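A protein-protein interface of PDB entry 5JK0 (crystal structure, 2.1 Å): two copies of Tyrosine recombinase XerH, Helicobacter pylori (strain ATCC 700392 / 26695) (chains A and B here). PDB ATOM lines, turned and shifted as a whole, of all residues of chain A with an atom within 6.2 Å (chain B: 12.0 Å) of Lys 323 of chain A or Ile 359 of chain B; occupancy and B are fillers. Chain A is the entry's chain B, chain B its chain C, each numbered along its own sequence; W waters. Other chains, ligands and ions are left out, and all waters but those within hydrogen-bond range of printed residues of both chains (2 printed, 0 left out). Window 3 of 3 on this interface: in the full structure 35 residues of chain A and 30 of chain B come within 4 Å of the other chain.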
ATOM      1  N   ASN A 178      38.033   4.681  16.837  1.00  0.00           N
ATOM      2  CA  ASN A 178      37.366   3.385  16.864  1.00  0.00           C
ATOM      3  C   ASN A 178      37.947   2.431  17.906  1.00  0.00           C
ATOM      4  O   ASN A 178      37.205   1.757  18.619  1.00  0.00           O
ATOM      5  CB  ASN A 178      37.426   2.735  15.482  1.00  0.00           C
ATOM      6  CG  ASN A 178      36.659   1.432  15.420  1.00  0.00           C
ATOM      7  OD1 ASN A 178      35.437   1.426  15.270  1.00  0.00           O
ATOM      8  ND2 ASN A 178      37.373   0.318  15.537  1.00  0.00           N
ATOM      9  N   PHE A 210      26.315   4.625  22.072  1.00  0.00           N
ATOM     10  CA  PHE A 210      25.726   3.982  20.903  1.00  0.00           C
ATOM     11  C   PHE A 210      24.836   4.907  20.075  1.00  0.00           C
ATOM     12  O   PHE A 210      24.603   4.650  18.893  1.00  0.00           O
ATOM     13  CB  PHE A 210      24.922   2.753  21.336  1.00  0.00           C
ATOM     14  CG  PHE A 210      25.774   1.605  21.797  1.00  0.00           C
ATOM     15  CD1 PHE A 210      26.933   1.272  21.117  1.00  0.00           C
ATOM     16  CD2 PHE A 210      25.422   0.866  22.914  1.00  0.00           C
ATOM     17  CE1 PHE A 210      27.721   0.220  21.537  1.00  0.00           C
ATOM     18  CE2 PHE A 210      26.206  -0.188  23.339  1.00  0.00           C
ATOM     19  CZ  PHE A 210      27.358  -0.511  22.650  1.00  0.00           C
ATOM     20  N   PHE A 316      30.834   9.584  18.401  1.00  0.00           N
ATOM     21  CA  PHE A 316      29.829   8.862  17.627  1.00  0.00           C
ATOM     22  C   PHE A 316      29.714   9.425  16.214  1.00  0.00           C
ATOM     23  O   PHE A 316      29.658   8.672  15.239  1.00  0.00           O
ATOM     24  CB  PHE A 316      28.466   8.915  18.327  1.00  0.00           C
ATOM     25  CG  PHE A 316      27.339   8.351  17.504  1.00  0.00           C
ATOM     26  CD1 PHE A 316      27.126   6.983  17.439  1.00  0.00           C
ATOM     27  CD2 PHE A 316      26.490   9.189  16.798  1.00  0.00           C
ATOM     28  CE1 PHE A 316      26.091   6.463  16.683  1.00  0.00           C
ATOM     29  CE2 PHE A 316      25.453   8.675  16.042  1.00  0.00           C
ATOM     30  CZ  PHE A 316      25.254   7.310  15.984  1.00  0.00           C
ATOM     31  N   THR A 318      31.937  11.131  14.524  1.00  0.00           N
ATOM     32  CA  THR A 318      33.170  10.887  13.782  1.00  0.00           C
ATOM     33  C   THR A 318      33.202   9.470  13.219  1.00  0.00           C
ATOM     34  O   THR A 318      33.573   9.256  12.063  1.00  0.00           O
ATOM     35  CB  THR A 318      34.411  11.109  14.666  1.00  0.00           C
ATOM     36  OG1 THR A 318      34.381  12.433  15.212  1.00  0.00           O
ATOM     37  CG2 THR A 318      35.686  10.926  13.856  1.00  0.00           C
ATOM     38  N   LEU A 319      32.802   8.507  14.043  1.00  0.00           N
ATOM     39  CA  LEU A 319      32.769   7.109  13.636  1.00  0.00           C
ATOM     40  C   LEU A 319      31.701   6.866  12.573  1.00  0.00           C
ATOM     41  O   LEU A 319      31.877   6.037  11.681  1.00  0.00           O
ATOM     42  CB  LEU A 319      32.515   6.208  14.848  1.00  0.00           C
ATOM     43  CG  LEU A 319      32.507   4.704  14.574  1.00  0.00           C
ATOM     44  CD1 LEU A 319      33.875   4.247  14.096  1.00  0.00           C
ATOM     45  CD2 LEU A 319      32.079   3.930  15.811  1.00  0.00           C
ATOM     46  N   LEU A 320      30.597   7.599  12.674  1.00  0.00           N
ATOM     47  CA  LEU A 320      29.478   7.426  11.755  1.00  0.00           C
ATOM     48  C   LEU A 320      29.844   7.841  10.332  1.00  0.00           C
ATOM     49  O   LEU A 320      29.474   7.167   9.371  1.00  0.00           O
ATOM     50  CB  LEU A 320      28.263   8.221  12.236  1.00  0.00           C
ATOM     51  CG  LEU A 320      27.008   8.097  11.370  1.00  0.00           C
ATOM     52  CD1 LEU A 320      26.661   6.633  11.135  1.00  0.00           C
ATOM     53  CD2 LEU A 320      25.838   8.831  12.009  1.00  0.00           C
ATOM     54  N   TYR A 321      30.568   8.947  10.199  1.00  0.00           N
ATOM     55  CA  TYR A 321      30.996   9.405   8.883  1.00  0.00           C
ATOM     56  C   TYR A 321      32.161   8.568   8.371  1.00  0.00           C
ATOM     57  O   TYR A 321      32.348   8.422   7.164  1.00  0.00           O
ATOM     58  CB  TYR A 321      31.393  10.883   8.914  1.00  0.00           C
ATOM     59  CG  TYR A 321      31.713  11.440   7.544  1.00  0.00           C
ATOM     60  CD1 TYR A 321      30.699  11.861   6.692  1.00  0.00           C
ATOM     61  CD2 TYR A 321      33.026  11.538   7.098  1.00  0.00           C
ATOM     62  CE1 TYR A 321      30.982  12.368   5.438  1.00  0.00           C
ATOM     63  CE2 TYR A 321      33.319  12.042   5.843  1.00  0.00           C
ATOM     64  CZ  TYR A 321      32.292  12.456   5.018  1.00  0.00           C
ATOM     65  OH  TYR A 321      32.574  12.961   3.768  1.00  0.00           O
ATOM     66  N   GLN A 322      32.944   8.024   9.295  1.00  0.00           N
ATOM     67  CA  GLN A 322      34.096   7.209   8.932  1.00  0.00           C
ATOM     68  C   GLN A 322      33.672   5.910   8.255  1.00  0.00           C
ATOM     69  O   GLN A 322      34.299   5.466   7.294  1.00  0.00           O
ATOM     70  CB  GLN A 322      34.939   6.896  10.170  1.00  0.00           C
ATOM     71  CG  GLN A 322      36.092   5.942   9.905  1.00  0.00           C
ATOM     72  CD  GLN A 322      36.700   5.395  11.179  1.00  0.00           C
ATOM     73  OE1 GLN A 322      36.273   5.736  12.282  1.00  0.00           O
ATOM     74  NE2 GLN A 322      37.703   4.537  11.034  1.00  0.00           N
ATOM     75  N   LYS A 323      32.599   5.311   8.759  1.00  0.00           N
ATOM     76  CA  LYS A 323      32.187   3.985   8.312  1.00  0.00           C
ATOM     77  C   LYS A 323      31.091   3.998   7.250  1.00  0.00           C
ATOM     78  O   LYS A 323      30.803   2.966   6.644  1.00  0.00           O
ATOM     79  CB  LYS A 323      31.724   3.153   9.510  1.00  0.00           C
ATOM     80  CG  LYS A 323      32.858   2.508  10.287  1.00  0.00           C
ATOM     81  CD  LYS A 323      32.329   1.608  11.389  1.00  0.00           C
ATOM     82  CE  LYS A 323      33.417   0.685  11.913  1.00  0.00           C
ATOM     83  NZ  LYS A 323      34.598   1.438  12.414  1.00  0.00           N
ATOM     84  N   ARG A 324      30.480   5.155   7.020  1.00  0.00           N
ATOM     85  CA  ARG A 324      29.372   5.227   6.073  1.00  0.00           C
ATOM     86  C   ARG A 324      29.558   6.314   5.017  1.00  0.00           C
ATOM     87  O   ARG A 324      28.964   6.239   3.940  1.00  0.00           O
ATOM     88  CB  ARG A 324      28.056   5.446   6.823  1.00  0.00           C
ATOM     89  CG  ARG A 324      27.588   4.227   7.607  1.00  0.00           C
ATOM     90  CD  ARG A 324      27.313   3.053   6.678  1.00  0.00           C
ATOM     91  NE  ARG A 324      26.820   1.881   7.396  1.00  0.00           N
ATOM     92  CZ  ARG A 324      27.579   0.856   7.772  1.00  0.00           C
ATOM     93  NH1 ARG A 324      28.876   0.849   7.495  1.00  0.00           N
ATOM     94  NH2 ARG A 324      27.040  -0.167   8.422  1.00  0.00           N
ATOM     95  N   HIS A 325      30.376   7.314   5.332  1.00  0.00           N
ATOM     96  CA  HIS A 325      30.667   8.418   4.416  1.00  0.00           C
ATOM     97  C   HIS A 325      29.385   9.101   3.944  1.00  0.00           C
ATOM     98  O   HIS A 325      29.286   9.541   2.799  1.00  0.00           O
ATOM     99  CB  HIS A 325      31.476   7.917   3.215  1.00  0.00           C
ATOM    100  CG  HIS A 325      32.280   8.985   2.539  1.00  0.00           C
ATOM    101  ND1 HIS A 325      33.423   9.520   3.095  1.00  0.00           N
ATOM    102  CD2 HIS A 325      32.107   9.617   1.353  1.00  0.00           C
ATOM    103  CE1 HIS A 325      33.919  10.435   2.281  1.00  0.00           C
ATOM    104  NE2 HIS A 325      33.140  10.513   1.217  1.00  0.00           N
ATOM    105  N   ARG B 352      16.612   4.788   6.534  1.00  0.00           N
ATOM    106  CA  ARG B 352      17.987   4.306   6.459  1.00  0.00           C
ATOM    107  C   ARG B 352      18.667   4.369   7.822  1.00  0.00           C
ATOM    108  O   ARG B 352      19.881   4.560   7.913  1.00  0.00           O
ATOM    109  CB  ARG B 352      18.786   5.119   5.439  1.00  0.00           C
ATOM    110  CG  ARG B 352      18.205   5.100   4.037  1.00  0.00           C
ATOM    111  CD  ARG B 352      19.055   5.911   3.068  1.00  0.00           C
ATOM    112  NE  ARG B 352      19.155   7.315   3.456  1.00  0.00           N
ATOM    113  CZ  ARG B 352      20.241   7.870   3.986  1.00  0.00           C
ATOM    114  NH1 ARG B 352      21.329   7.143   4.189  1.00  0.00           N
ATOM    115  NH2 ARG B 352      20.239   9.157   4.309  1.00  0.00           N
ATOM    116  N   LEU B 353      17.880   4.204   8.878  1.00  0.00           N
ATOM    117  CA  LEU B 353      18.399   4.292  10.237  1.00  0.00           C
ATOM    118  C   LEU B 353      19.167   3.030  10.631  1.00  0.00           C
ATOM    119  O   LEU B 353      19.974   3.053  11.561  1.00  0.00           O
ATOM    120  CB  LEU B 353      17.260   4.551  11.224  1.00  0.00           C
ATOM    121  N   GLU B 354      18.912   1.932   9.923  1.00  0.00           N
ATOM    122  CA  GLU B 354      19.648   0.692  10.155  1.00  0.00           C
ATOM    123  C   GLU B 354      21.084   0.817   9.661  1.00  0.00           C
ATOM    124  O   GLU B 354      21.988   0.151  10.169  1.00  0.00           O
ATOM    125  CB  GLU B 354      18.965  -0.491   9.465  1.00  0.00           C
ATOM    126  CG  GLU B 354      17.658  -0.937  10.103  1.00  0.00           C
ATOM    127  CD  GLU B 354      16.451  -0.205   9.549  1.00  0.00           C
ATOM    128  OE1 GLU B 354      15.322  -0.714   9.714  1.00  0.00           O
ATOM    129  OE2 GLU B 354      16.629   0.875   8.947  1.00  0.00           O
ATOM    130  N   GLU B 355      21.284   1.678   8.669  1.00  0.00           N
ATOM    131  CA  GLU B 355      22.602   1.885   8.079  1.00  0.00           C
ATOM    132  C   GLU B 355      23.555   2.570   9.054  1.00  0.00           C
ATOM    133  O   GLU B 355      24.773   2.469   8.918  1.00  0.00           O
ATOM    134  CB  GLU B 355      22.486   2.709   6.793  1.00  0.00           C
ATOM    135  N   ALA B 356      22.994   3.266  10.036  1.00  0.00           N
ATOM    136  CA  ALA B 356      23.797   3.974  11.026  1.00  0.00           C
ATOM    137  C   ALA B 356      23.960   3.153  12.302  1.00  0.00           C
ATOM    138  O   ALA B 356      24.871   3.395  13.093  1.00  0.00           O
ATOM    139  CB  ALA B 356      23.174   5.324  11.342  1.00  0.00           C
ATOM    140  N   ALA B 357      23.073   2.182  12.494  1.00  0.00           N
ATOM    141  CA  ALA B 357      23.076   1.367  13.703  1.00  0.00           C
ATOM    142  C   ALA B 357      24.023   0.175  13.584  1.00  0.00           C
ATOM    143  O   ALA B 357      24.392  -0.437  14.587  1.00  0.00           O
ATOM    144  CB  ALA B 357      21.666   0.887  14.016  1.00  0.00           C
ATOM    145  N   SER B 358      24.418  -0.144  12.357  1.00  0.00           N
ATOM    146  CA  SER B 358      25.248  -1.316  12.102  1.00  0.00           C
ATOM    147  C   SER B 358      26.736  -0.983  12.072  1.00  0.00           C
ATOM    148  O   SER B 358      27.551  -1.792  11.629  1.00  0.00           O
ATOM    149  CB  SER B 358      24.837  -1.973  10.782  1.00  0.00           C
ATOM    150  OG  SER B 358      24.941  -1.057   9.705  1.00  0.00           O
ATOM    151  N   ILE B 359      27.090   0.207  12.547  1.00  0.00           N
ATOM    152  CA  ILE B 359      28.481   0.650  12.531  1.00  0.00           C
ATOM    153  C   ILE B 359      29.291   0.027  13.665  1.00  0.00           C
ATOM    154  O   ILE B 359      30.517   0.119  13.684  1.00  0.00           O
ATOM    155  CB  ILE B 359      28.588   2.185  12.629  1.00  0.00           C
ATOM    156  CG1 ILE B 359      28.024   2.680  13.964  1.00  0.00           C
ATOM    157  CG2 ILE B 359      27.872   2.847  11.460  1.00  0.00           C
ATOM    158  CD1 ILE B 359      28.152   4.174  14.163  1.00  0.00           C
ATOM    159  N   TRP B 360      28.601  -0.605  14.608  1.00  0.00           N
ATOM    160  CA  TRP B 360      29.267  -1.216  15.754  1.00  0.00           C
ATOM    161  C   TRP B 360      29.586  -2.686  15.501  1.00  0.00           C
ATOM    162  O   TRP B 360      30.059  -3.392  16.394  1.00  0.00           O
ATOM    163  CB  TRP B 360      28.402  -1.076  17.009  1.00  0.00           C
ATOM    164  CG  TRP B 360      28.101   0.345  17.373  1.00  0.00           C
ATOM    165  CD1 TRP B 360      26.935   1.017  17.156  1.00  0.00           C
ATOM    166  CD2 TRP B 360      28.985   1.271  18.015  1.00  0.00           C
ATOM    167  NE1 TRP B 360      27.036   2.304  17.627  1.00  0.00           N
ATOM    168  CE2 TRP B 360      28.285   2.486  18.158  1.00  0.00           C
ATOM    169  CE3 TRP B 360      30.301   1.192  18.482  1.00  0.00           C
ATOM    170  CZ2 TRP B 360      28.856   3.611  18.749  1.00  0.00           C
ATOM    171  CZ3 TRP B 360      30.865   2.309  19.068  1.00  0.00           C
ATOM    172  CH2 TRP B 360      30.144   3.503  19.196  1.00  0.00           C
ATOM    173  N   GLU B 361      29.330  -3.142  14.279  1.00  0.00           N
ATOM    174  CA  GLU B 361      29.505  -4.546  13.930  1.00  0.00           C
ATOM    175  C   GLU B 361      30.464  -4.720  12.756  1.00  0.00           C
ATOM    176  O   GLU B 361      30.459  -3.927  11.815  1.00  0.00           O
ATOM    177  CB  GLU B 361      28.151  -5.177  13.605  1.00  0.00           C
ATOM    178  CG  GLU B 361      27.091  -4.928  14.667  1.00  0.00           C
ATOM    179  CD  GLU B 361      25.692  -5.260  14.188  1.00  0.00           C
ATOM    180  OE1 GLU B 361      25.555  -6.142  13.315  1.00  0.00           O
ATOM    181  OE2 GLU B 361      24.731  -4.633  14.680  1.00  0.00           O
HETATM  182  O   HOH W   1      30.293  -1.777   9.202  1.00  0.00           O
HETATM  183  O   HOH W   2      23.751   2.865  17.078  1.00  0.00           O
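O of Glu 355 of chain B lies within hydrogen-bond range of NE of Arg 324 of chain A.
NH2 of Arg 324 of chain A is in hydrogen-bond range of OG of Ser 358 of chain B (2.6 Å).
The side-chain amino group (NZ) of Lys 323 of chain A is in hydrogen-bond range of the side-chain amide oxygen (OD1) of Asn 178 of chain A (3.0 Å).
The side-chain hydroxyl (OG) of Ser 358 of chain B is in hydrogen-bond range of the backbone carbonyl oxygen (O) of Glu 354 of chain B (3.2 Å).
Among the printed residues, merely in contact across the chains: Phe 210 of chain A with Trp 360 of chain B, Phe 316 of chain A with Ile 359 of chain B, Leu 319 of chain A with Trp 360 of chain B, Leu 320 of chain A with Ala 356 of chain B, Leu 320 of chain A with Ile 359 of chain B and Lys 323 of chain A with Ile 359 of chain B.
No residue of chain B comes within 4 Å of Asn 178 of chain A.
Printed residues of chain B within 4 Å of Phe 210 of chain A: Trp 360 (3.5 Å).
Of the printed residues of chain B, Phe 316 of chain A touches Ile 359 (3.98 Å).
Leu 319 of chain A touches just one residue of chain B: Trp 360.
No residue of chain B comes within 4 Å of Gln 322 of chain A.
Lys 323 of chain A touches one residue of chain B.
Arg 324 of chain A touches two residues of chain B.
Of the printed residues of chain A, Ala 356 of chain B touches Leu 320 (3.7 Å).
Of the printed residues of chain A, Ile 359 of chain B touches Phe 316 (3.98 Å), Leu 320 (3.99 Å) and Lys 323 (3.3 Å).
Of the printed residues of chain A, Trp 360 of chain B touches Phe 210 (3.5 Å) and Leu 319 (3.8 Å).
The nearest residue of chain B that does not touch Lys 323 of chain A is Trp 360 of chain B (5.4 Å).
The nearest printed residue of chain B that does not touch Leu 320 of chain A is Glu 355 of chain B (5.1 Å).
Along chain B the printed residues that touch a printed residue of chain A span positions 355 to 360.
Among the printed residues, 8 pairs touch across the chains.
Among the printed residues, no Asp or Glu carboxylate lies within 4 Å of a Lys or Arg side-chain nitrogen of the other chain.
No position is printed for both chains.
Of the 8 pairs that touch across the chains among the printed residues, none has its exchanged pair printed and touching as well.
Water W2 lies within hydrogen-bond range of O of Phe 210 of chain A (2.7 Å) and NE1 of Trp 360 of chain B (3.4 Å).
Water W1 lies within hydrogen-bond range of O of Glu 361 of chain B (3.4 Å) and NH1 of Arg 324 of chain A (3.4 Å).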
